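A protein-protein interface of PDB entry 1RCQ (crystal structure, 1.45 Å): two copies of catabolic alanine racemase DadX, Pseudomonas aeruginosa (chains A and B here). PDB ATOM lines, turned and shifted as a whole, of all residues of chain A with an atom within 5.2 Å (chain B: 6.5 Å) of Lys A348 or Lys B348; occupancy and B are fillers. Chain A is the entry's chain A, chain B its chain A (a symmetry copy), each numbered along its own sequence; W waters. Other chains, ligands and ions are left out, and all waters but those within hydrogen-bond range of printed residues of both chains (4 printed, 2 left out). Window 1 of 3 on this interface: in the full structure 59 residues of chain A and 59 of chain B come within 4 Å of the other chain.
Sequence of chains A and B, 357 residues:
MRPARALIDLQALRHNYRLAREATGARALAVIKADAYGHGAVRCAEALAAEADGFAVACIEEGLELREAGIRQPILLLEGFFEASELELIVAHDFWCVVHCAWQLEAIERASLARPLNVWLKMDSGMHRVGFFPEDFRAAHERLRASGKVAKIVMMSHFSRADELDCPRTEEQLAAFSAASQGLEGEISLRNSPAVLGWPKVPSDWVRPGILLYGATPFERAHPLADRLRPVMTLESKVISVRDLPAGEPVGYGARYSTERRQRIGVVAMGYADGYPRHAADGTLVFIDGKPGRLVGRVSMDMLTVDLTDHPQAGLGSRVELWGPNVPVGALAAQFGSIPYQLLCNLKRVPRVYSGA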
ATOM      1  N   GLY A  38       9.243 -16.715  -0.690  1.00  0.00           N
ATOM      2  CA  GLY A  38       9.573 -18.045  -0.314  1.00  0.00           C
ATOM      3  C   GLY A  38       9.292 -19.197  -1.251  1.00  0.00           C
ATOM      4  O   GLY A  38       9.662 -20.340  -0.937  1.00  0.00           O
ATOM      5  N   ALA A 273      11.898 -23.802  12.546  1.00  0.00           N
ATOM      6  CA  ALA A 273      13.048 -23.478  11.705  1.00  0.00           C
ATOM      7  C   ALA A 273      12.668 -23.618  10.225  1.00  0.00           C
ATOM      8  O   ALA A 273      13.273 -22.976   9.358  1.00  0.00           O
ATOM      9  CB  ALA A 273      14.231 -24.400  11.996  1.00  0.00           C
ATOM     10  N   ASP A 274      11.689 -24.474   9.943  1.00  0.00           N
ATOM     11  CA  ASP A 274      11.175 -24.650   8.596  1.00  0.00           C
ATOM     12  C   ASP A 274      10.264 -23.519   8.140  1.00  0.00           C
ATOM     13  O   ASP A 274       9.967 -23.414   6.922  1.00  0.00           O
ATOM     14  CB  ASP A 274      10.418 -25.984   8.457  1.00  0.00           C
ATOM     15  CG  ASP A 274      11.279 -27.125   8.928  1.00  0.00           C
ATOM     16  OD1 ASP A 274      12.222 -27.504   8.209  1.00  0.00           O
ATOM     17  OD2 ASP A 274      10.985 -27.611  10.034  1.00  0.00           O
ATOM     18  N   GLY A 275       9.797 -22.693   9.075  1.00  0.00           N
ATOM     19  CA  GLY A 275       8.873 -21.606   8.786  1.00  0.00           C
ATOM     20  C   GLY A 275       7.501 -21.798   9.390  1.00  0.00           C
ATOM     21  O   GLY A 275       6.646 -20.915   9.287  1.00  0.00           O
ATOM     22  N   LEU A 344       5.031 -17.459   4.557  1.00  0.00           N
ATOM     23  CA  LEU A 344       5.552 -17.911   3.267  1.00  0.00           C
ATOM     24  C   LEU A 344       7.021 -17.515   3.118  1.00  0.00           C
ATOM     25  O   LEU A 344       7.874 -18.324   2.735  1.00  0.00           O
ATOM     26  CB  LEU A 344       4.666 -17.342   2.166  1.00  0.00           C
ATOM     27  CG  LEU A 344       3.209 -17.833   2.207  1.00  0.00           C
ATOM     28  CD1 LEU A 344       2.325 -17.031   1.281  1.00  0.00           C
ATOM     29  CD2 LEU A 344       3.113 -19.326   1.872  1.00  0.00           C
ATOM     30  N   CYS A 345       7.378 -16.268   3.437  1.00  0.00           N
ATOM     31  CA  CYS A 345       8.763 -15.835   3.342  1.00  0.00           C
ATOM     32  C   CYS A 345       9.719 -16.587   4.274  1.00  0.00           C
ATOM     33  O   CYS A 345      10.920 -16.682   3.955  1.00  0.00           O
ATOM     34  CB  CYS A 345       8.906 -14.344   3.654  1.00  0.00           C
ATOM     35  SG  CYS A 345       8.418 -13.226   2.311  1.00  0.00           S
ATOM     36  N   ASN A 346       9.209 -17.118   5.370  1.00  0.00           N
ATOM     37  CA  ASN A 346      10.047 -17.775   6.371  1.00  0.00           C
ATOM     38  C   ASN A 346      10.373 -19.198   5.962  1.00  0.00           C
ATOM     39  O   ASN A 346      11.113 -19.870   6.689  1.00  0.00           O
ATOM     40  CB  ASN A 346       9.360 -17.812   7.746  1.00  0.00           C
ATOM     41  CG  ASN A 346       9.343 -16.488   8.486  1.00  0.00           C
ATOM     42  OD1 ASN A 346      10.138 -15.552   8.272  1.00  0.00           O
ATOM     43  ND2 ASN A 346       8.402 -16.445   9.392  1.00  0.00           N
ATOM     44  N   LEU A 347       9.870 -19.681   4.835  1.00  0.00           N
ATOM     45  CA  LEU A 347      10.128 -21.065   4.450  1.00  0.00           C
ATOM     46  C   LEU A 347      11.622 -21.319   4.301  1.00  0.00           C
ATOM     47  O   LEU A 347      12.293 -20.601   3.580  1.00  0.00           O
ATOM     48  CB  LEU A 347       9.400 -21.431   3.148  1.00  0.00           C
ATOM     49  CG  LEU A 347       9.461 -22.912   2.791  1.00  0.00           C
ATOM     50  CD1 LEU A 347       8.535 -23.781   3.651  1.00  0.00           C
ATOM     51  CD2 LEU A 347       9.115 -23.116   1.329  1.00  0.00           C
ATOM     52  N   LYS A 348      12.080 -22.342   5.015  1.00  0.00           N
ATOM     53  CA  LYS A 348      13.474 -22.780   4.986  1.00  0.00           C
ATOM     54  C   LYS A 348      13.596 -24.309   5.076  1.00  0.00           C
ATOM     55  O   LYS A 348      12.652 -24.976   5.521  1.00  0.00           O
ATOM     56  CB  LYS A 348      14.295 -22.171   6.135  1.00  0.00           C
ATOM     57  CG  LYS A 348      14.480 -20.673   6.104  1.00  0.00           C
ATOM     58  CD  LYS A 348      15.422 -20.150   7.172  1.00  0.00           C
ATOM     59  CE  LYS A 348      16.874 -20.547   7.012  1.00  0.00           C
ATOM     60  NZ  LYS A 348      17.748 -19.932   8.061  1.00  0.00           N
ATOM     61  N   ARG A 349      14.752 -24.828   4.719  1.00  0.00           N
ATOM     62  CA  ARG A 349      15.241 -26.185   4.936  1.00  0.00           C
ATOM     63  C   ARG A 349      14.507 -27.225   4.113  1.00  0.00           C
ATOM     64  O   ARG A 349      15.175 -28.057   3.474  1.00  0.00           O
ATOM     65  CB  ARG A 349      15.164 -26.590   6.417  1.00  0.00           C
ATOM     66  CG  ARG A 349      15.719 -27.982   6.663  1.00  0.00           C
ATOM     67  CD  ARG A 349      16.117 -28.210   8.114  1.00  0.00           C
ATOM     68  NE  ARG A 349      14.975 -28.012   9.002  1.00  0.00           N
ATOM     69  CZ  ARG A 349      15.053 -28.116  10.318  1.00  0.00           C
ATOM     70  NH1 ARG A 349      16.195 -28.434  10.923  1.00  0.00           N
ATOM     71  NH2 ARG A 349      13.949 -27.901  11.038  1.00  0.00           N
ATOM     72  N   VAL A 350      13.163 -27.176   4.108  1.00  0.00           N
ATOM     73  CA  VAL A 350      12.458 -28.247   3.416  1.00  0.00           C
ATOM     74  C   VAL A 350      12.609 -28.203   1.904  1.00  0.00           C
ATOM     75  O   VAL A 350      12.770 -27.127   1.333  1.00  0.00           O
ATOM     76  CB  VAL A 350      10.965 -28.222   3.776  1.00  0.00           C
ATOM     77  CG1 VAL A 350      10.905 -28.298   5.303  1.00  0.00           C
ATOM     78  CG2 VAL A 350      10.251 -27.013   3.212  1.00  0.00           C
ATOM     79  N   ARG B   2      22.461  -4.136  -1.538  1.00  0.00           N
ATOM     80  CA  ARG B   2      21.785  -3.840  -0.296  1.00  0.00           C
ATOM     81  C   ARG B   2      22.707  -3.944   0.918  1.00  0.00           C
ATOM     82  O   ARG B   2      23.475  -4.905   1.023  1.00  0.00           O
ATOM     83  CB  ARG B   2      20.682  -4.869  -0.212  1.00  0.00           C
ATOM     84  CG  ARG B   2      19.542  -4.591   0.719  1.00  0.00           C
ATOM     85  CD  ARG B   2      18.435  -5.626   0.462  1.00  0.00           C
ATOM     86  NE  ARG B   2      17.444  -5.572   1.551  1.00  0.00           N
ATOM     87  CZ  ARG B   2      17.173  -6.518   2.446  1.00  0.00           C
ATOM     88  NH1 ARG B   2      17.806  -7.700   2.488  1.00  0.00           N
ATOM     89  NH2 ARG B   2      16.230  -6.280   3.343  1.00  0.00           N
ATOM     90  N   ALA B  34      19.367 -27.243  12.197  1.00  0.00           N
ATOM     91  CA  ALA B  34      18.779 -26.085  11.528  1.00  0.00           C
ATOM     92  C   ALA B  34      19.836 -25.075  11.064  1.00  0.00           C
ATOM     93  O   ALA B  34      19.721 -23.860  11.275  1.00  0.00           O
ATOM     94  CB  ALA B  34      17.735 -25.416  12.419  1.00  0.00           C
ATOM     95  N   ASP B  35      20.877 -25.569  10.399  1.00  0.00           N
ATOM     96  CA  ASP B  35      21.951 -24.740   9.874  1.00  0.00           C
ATOM     97  C   ASP B  35      22.601 -23.930  10.989  1.00  0.00           C
ATOM     98  O   ASP B  35      22.806 -22.726  10.853  1.00  0.00           O
ATOM     99  CB  ASP B  35      21.417 -23.874   8.709  1.00  0.00           C
ATOM    100  CG  ASP B  35      22.546 -23.341   7.870  1.00  0.00           C
ATOM    101  OD1 ASP B  35      23.566 -24.057   7.765  1.00  0.00           O
ATOM    102  OD2 ASP B  35      22.426 -22.220   7.340  1.00  0.00           O
ATOM    103  N   TYR B  37      21.296 -23.145  13.876  1.00  0.00           N
ATOM    104  CA  TYR B  37      20.305 -22.156  14.282  1.00  0.00           C
ATOM    105  C   TYR B  37      20.421 -20.894  13.442  1.00  0.00           C
ATOM    106  O   TYR B  37      20.402 -19.767  13.936  1.00  0.00           O
ATOM    107  CB  TYR B  37      20.435 -21.767  15.753  1.00  0.00           C
ATOM    108  CG  TYR B  37      20.155 -22.831  16.773  1.00  0.00           C
ATOM    109  CD1 TYR B  37      20.244 -24.190  16.511  1.00  0.00           C
ATOM    110  CD2 TYR B  37      19.783 -22.451  18.073  1.00  0.00           C
ATOM    111  CE1 TYR B  37      19.977 -25.128  17.515  1.00  0.00           C
ATOM    112  CE2 TYR B  37      19.525 -23.378  19.065  1.00  0.00           C
ATOM    113  CZ  TYR B  37      19.619 -24.729  18.784  1.00  0.00           C
ATOM    114  OH  TYR B  37      19.357 -25.679  19.756  1.00  0.00           O
ATOM    115  N   GLY B  38      20.578 -21.046  12.127  1.00  0.00           N
ATOM    116  CA  GLY B  38      20.760 -19.976  11.211  1.00  0.00           C
ATOM    117  C   GLY B  38      22.131 -19.376  10.998  1.00  0.00           C
ATOM    118  O   GLY B  38      22.281 -18.496  10.134  1.00  0.00           O
ATOM    119  N   ALA B 273      11.403 -10.659   5.773  1.00  0.00           N
ATOM    120  CA  ALA B 273      11.834 -11.783   4.946  1.00  0.00           C
ATOM    121  C   ALA B 273      13.271 -12.179   5.310  1.00  0.00           C
ATOM    122  O   ALA B 273      13.674 -13.331   5.112  1.00  0.00           O
ATOM    123  CB  ALA B 273      11.784 -11.435   3.459  1.00  0.00           C
ATOM    124  N   ASP B 274      14.041 -11.217   5.813  1.00  0.00           N
ATOM    125  CA  ASP B 274      15.396 -11.466   6.272  1.00  0.00           C
ATOM    126  C   ASP B 274      15.461 -12.169   7.620  1.00  0.00           C
ATOM    127  O   ASP B 274      16.548 -12.674   8.005  1.00  0.00           O
ATOM    128  CB  ASP B 274      16.208 -10.161   6.352  1.00  0.00           C
ATOM    129  CG  ASP B 274      16.141  -9.421   5.043  1.00  0.00           C
ATOM    130  OD1 ASP B 274      16.796  -9.851   4.076  1.00  0.00           O
ATOM    131  OD2 ASP B 274      15.410  -8.417   5.019  1.00  0.00           O
ATOM    132  N   GLY B 275      14.349 -12.196   8.353  1.00  0.00           N
ATOM    133  CA  GLY B 275      14.287 -12.783   9.683  1.00  0.00           C
ATOM    134  C   GLY B 275      14.046 -11.774  10.782  1.00  0.00           C
ATOM    135  O   GLY B 275      13.893 -12.148  11.947  1.00  0.00           O
ATOM    136  N   LEU B 344      16.882 -16.299  15.228  1.00  0.00           N
ATOM    137  CA  LEU B 344      18.143 -16.749  14.637  1.00  0.00           C
ATOM    138  C   LEU B 344      17.877 -17.754  13.517  1.00  0.00           C
ATOM    139  O   LEU B 344      18.429 -17.657  12.416  1.00  0.00           O
ATOM    140  CB  LEU B 344      19.018 -17.313  15.749  1.00  0.00           C
ATOM    141  CG  LEU B 344      19.419 -16.287  16.822  1.00  0.00           C
ATOM    142  CD1 LEU B 344      20.039 -16.956  18.027  1.00  0.00           C
ATOM    143  CD2 LEU B 344      20.371 -15.227  16.255  1.00  0.00           C
ATOM    144  N   CYS B 345      17.004 -18.740  13.742  1.00  0.00           N
ATOM    145  CA  CYS B 345      16.687 -19.713  12.709  1.00  0.00           C
ATOM    146  C   CYS B 345      16.028 -19.112  11.463  1.00  0.00           C
ATOM    147  O   CYS B 345      16.165 -19.695  10.370  1.00  0.00           O
ATOM    148  CB  CYS B 345      15.750 -20.803  13.235  1.00  0.00           C
ATOM    149  SG  CYS B 345      16.544 -22.077  14.255  1.00  0.00           S
ATOM    150  N   ASN B 346      15.359 -17.984  11.612  1.00  0.00           N
ATOM    151  CA  ASN B 346      14.617 -17.376  10.510  1.00  0.00           C
ATOM    152  C   ASN B 346      15.538 -16.584   9.603  1.00  0.00           C
ATOM    153  O   ASN B 346      15.063 -16.046   8.596  1.00  0.00           O
ATOM    154  CB  ASN B 346      13.516 -16.434  11.022  1.00  0.00           C
ATOM    155  CG  ASN B 346      12.294 -17.131  11.590  1.00  0.00           C
ATOM    156  OD1 ASN B 346      11.961 -18.300  11.316  1.00  0.00           O
ATOM    157  ND2 ASN B 346      11.616 -16.354  12.393  1.00  0.00           N
ATOM    158  N   LEU B 347      16.827 -16.499   9.900  1.00  0.00           N
ATOM    159  CA  LEU B 347      17.721 -15.698   9.069  1.00  0.00           C
ATOM    160  C   LEU B 347      17.729 -16.204   7.633  1.00  0.00           C
ATOM    161  O   LEU B 347      17.959 -17.379   7.402  1.00  0.00           O
ATOM    162  CB  LEU B 347      19.150 -15.688   9.630  1.00  0.00           C
ATOM    163  CG  LEU B 347      20.091 -14.713   8.930  1.00  0.00           C
ATOM    164  CD1 LEU B 347      19.841 -13.249   9.311  1.00  0.00           C
ATOM    165  CD2 LEU B 347      21.535 -15.065   9.234  1.00  0.00           C
ATOM    166  N   LYS B 348      17.458 -15.276   6.721  1.00  0.00           N
ATOM    167  CA  LYS B 348      17.453 -15.542   5.283  1.00  0.00           C
ATOM    168  C   LYS B 348      18.007 -14.355   4.481  1.00  0.00           C
ATOM    169  O   LYS B 348      18.044 -13.228   4.994  1.00  0.00           O
ATOM    170  CB  LYS B 348      16.041 -15.852   4.758  1.00  0.00           C
ATOM    171  CG  LYS B 348      15.400 -17.119   5.271  1.00  0.00           C
ATOM    172  CD  LYS B 348      14.078 -17.449   4.604  1.00  0.00           C
ATOM    173  CE  LYS B 348      14.163 -17.830   3.142  1.00  0.00           C
ATOM    174  NZ  LYS B 348      12.830 -18.214   2.577  1.00  0.00           N
ATOM    175  N   ARG B 349      18.366 -14.603   3.238  1.00  0.00           N
ATOM    176  CA  ARG B 349      18.676 -13.650   2.178  1.00  0.00           C
ATOM    177  C   ARG B 349      19.968 -12.893   2.412  1.00  0.00           C
ATOM    178  O   ARG B 349      20.788 -12.814   1.481  1.00  0.00           O
ATOM    179  CB  ARG B 349      17.542 -12.633   1.975  1.00  0.00           C
ATOM    180  CG  ARG B 349      17.830 -11.667   0.839  1.00  0.00           C
ATOM    181  CD  ARG B 349      16.574 -11.004   0.295  1.00  0.00           C
ATOM    182  NE  ARG B 349      15.877 -10.272   1.347  1.00  0.00           N
ATOM    183  CZ  ARG B 349      14.737  -9.630   1.153  1.00  0.00           C
ATOM    184  NH1 ARG B 349      14.156  -9.596  -0.045  1.00  0.00           N
ATOM    185  NH2 ARG B 349      14.176  -9.003   2.189  1.00  0.00           N
ATOM    186  N   VAL B 350      20.162 -12.359   3.632  1.00  0.00           N
ATOM    187  CA  VAL B 350      21.345 -11.531   3.818  1.00  0.00           C
ATOM    188  C   VAL B 350      22.650 -12.311   3.794  1.00  0.00           C
ATOM    189  O   VAL B 350      22.673 -13.481   4.170  1.00  0.00           O
ATOM    190  CB  VAL B 350      21.248 -10.750   5.137  1.00  0.00           C
ATOM    191  CG1 VAL B 350      19.929  -9.977   5.064  1.00  0.00           C
ATOM    192  CG2 VAL B 350      21.345 -11.647   6.352  1.00  0.00           C
ATOM    193  N   PRO B 351      23.726 -11.660   3.386  1.00  0.00           N
ATOM    194  CA  PRO B 351      25.015 -12.340   3.508  1.00  0.00           C
ATOM    195  C   PRO B 351      25.399 -12.608   4.960  1.00  0.00           C
ATOM    196  O   PRO B 351      25.092 -11.813   5.822  1.00  0.00           O
ATOM    197  CB  PRO B 351      26.015 -11.357   2.886  1.00  0.00           C
ATOM    198  CG  PRO B 351      25.264 -10.280   2.241  1.00  0.00           C
ATOM    199  CD  PRO B 351      23.844 -10.320   2.792  1.00  0.00           C
ATOM    200  N   ARG B 352      26.116 -13.732   5.167  1.00  0.00           N
ATOM    201  CA  ARG B 352      26.708 -14.081   6.439  1.00  0.00           C
ATOM    202  C   ARG B 352      28.226 -13.933   6.276  1.00  0.00           C
ATOM    203  O   ARG B 352      28.825 -14.577   5.423  1.00  0.00           O
ATOM    204  CB  ARG B 352      26.352 -15.497   6.892  1.00  0.00           C
ATOM    205  CG  ARG B 352      24.889 -15.635   7.341  1.00  0.00           C
ATOM    206  CD  ARG B 352      24.477 -17.037   7.739  1.00  0.00           C
ATOM    207  NE  ARG B 352      24.695 -17.946   6.610  1.00  0.00           N
ATOM    208  CZ  ARG B 352      24.256 -19.184   6.596  1.00  0.00           C
ATOM    209  NH1 ARG B 352      23.577 -19.632   7.638  1.00  0.00           N
ATOM    210  NH2 ARG B 352      24.440 -20.029   5.602  1.00  0.00           N
HETATM  211  O   HOH W   1      11.876 -15.707   1.352  1.00  0.00           O
HETATM  212  O   HOH W   2       8.872 -15.823  12.093  1.00  0.00           O
HETATM  213  O   HOH W   3      20.172 -21.141   6.917  1.00  0.00           O
HETATM  214  O   HOH W   4      17.918 -22.040  10.114  1.00  0.00           O
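The backbone carbonyl oxygen (O) of Cys A345 lies within hydrogen-bond range of the side-chain amino group (NZ) of Lys B348.
NZ of Lys A348 is in hydrogen-bond range of O of Cys B345, 2.8 Å away.
The backbone carbonyl oxygen of Leu A347 sits at hydrogen-bond distance from the side-chain amino group of Lys B348, at 2.6 Å.
O of Leu B347 lies within hydrogen-bond range of NZ of Lys A348, at 2.6 Å.
The side-chain carboxylate (OD1) of Asp A274 is in salt-bridge range of the guanidinium group (NE) of Arg A349 (2.9 Å).
The backbone carbonyl oxygen (O) of Asp B274 lies within hydrogen-bond range of the backbone NH (N) of Lys B348, at 3.0 Å.
The backbone carbonyl oxygen of Asp A274 lies within hydrogen-bond range of the backbone NH of Lys A348, at 3.0 Å.
Among the printed residues, pairs that only touch across the chains: Arg A349 with Ala B34 (3.5 Å), Lys A348 with Lys B348 (3.6 Å), Ala A273 with Ala B34 (3.7 Å), Ala A273 with Cys B345 (3.98 Å) and Cys A345 with Ala B273 (3.98 Å).
Printed residues of chain B within 4 Å of Cys A345: Ala B273 and Lys B348.
Of the printed residues of chain B, Leu A347 touches Lys B348.
Of the printed residues of chain B, Lys A348 touches Cys B345 (2.8 Å), Leu B347 (2.6 Å) and Lys B348 (3.6 Å).
Of the printed residues of chain B, Arg A349 touches Ala B34 (3.5 Å).
Printed residues of chain A within 4 Å of Cys B345: Ala A273 and Lys A348.
Lys B348 touches just these residues of chain A: Cys A345 (2.8 Å), Leu A347 (2.6 Å) and Lys A348 (3.6 Å).
Val B350 touches none of the printed residues of chain A.
The nearest residue of chain A that does not touch Lys B348 is Asn A346 (4.3 Å).
Hydrophobic or aromatic side chains of chain A that line the printed part of chain B: Ala A273.
Of the 17 printed residues of chain B, 5 touch a printed residue of chain A.
Hydrophobic or aromatic side chains of chain B within 4 Å of the printed part of chain A: Ala B34 and Ala B273.
Among the printed residues, 9 pairs touch across the chains.
Among the printed residues, no Asp or Glu carboxylate lies within 4 Å of a Lys or Arg side-chain nitrogen of the other chain.
Ala A273 touches Cys B345, and with the chains exchanged Cys A345 touches Ala B273.
Cys A345 touches Lys B348, and with the chains exchanged Lys A348 touches Cys B345.
Leu A347 touches Lys B348, and with the chains exchanged Lys A348 touches Leu B347.
Lys A348 touches its own counterpart, Lys B348.
11 positions are printed for both chains.
Water W3 lies within hydrogen-bond range of OD2 of Asp B35 (2.5 Å) and NZ of Lys A348 (2.9 Å).
Water W2 bridges ND2 of Asn B346 (2.8 Å) and ND2 of Asn A346 (2.8 Å).
Water W4 lies within hydrogen-bond range of the backbone carbonyl oxygen (O) of Ala B34 (2.8 Å), the backbone carbonyl oxygen (O) of Cys B345 (2.9 Å), the side-chain amino group (NZ) of Lys A348 (2.9 Å) and the backbone NH (N) of Gly B38 (3.5 Å).
Water W1 lies within hydrogen-bond range of the backbone carbonyl oxygen of Cys A345 (2.9 Å), the side-chain amino group of Lys B348 (2.9 Å) and the backbone NH of Gly A38 (3.5 Å).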
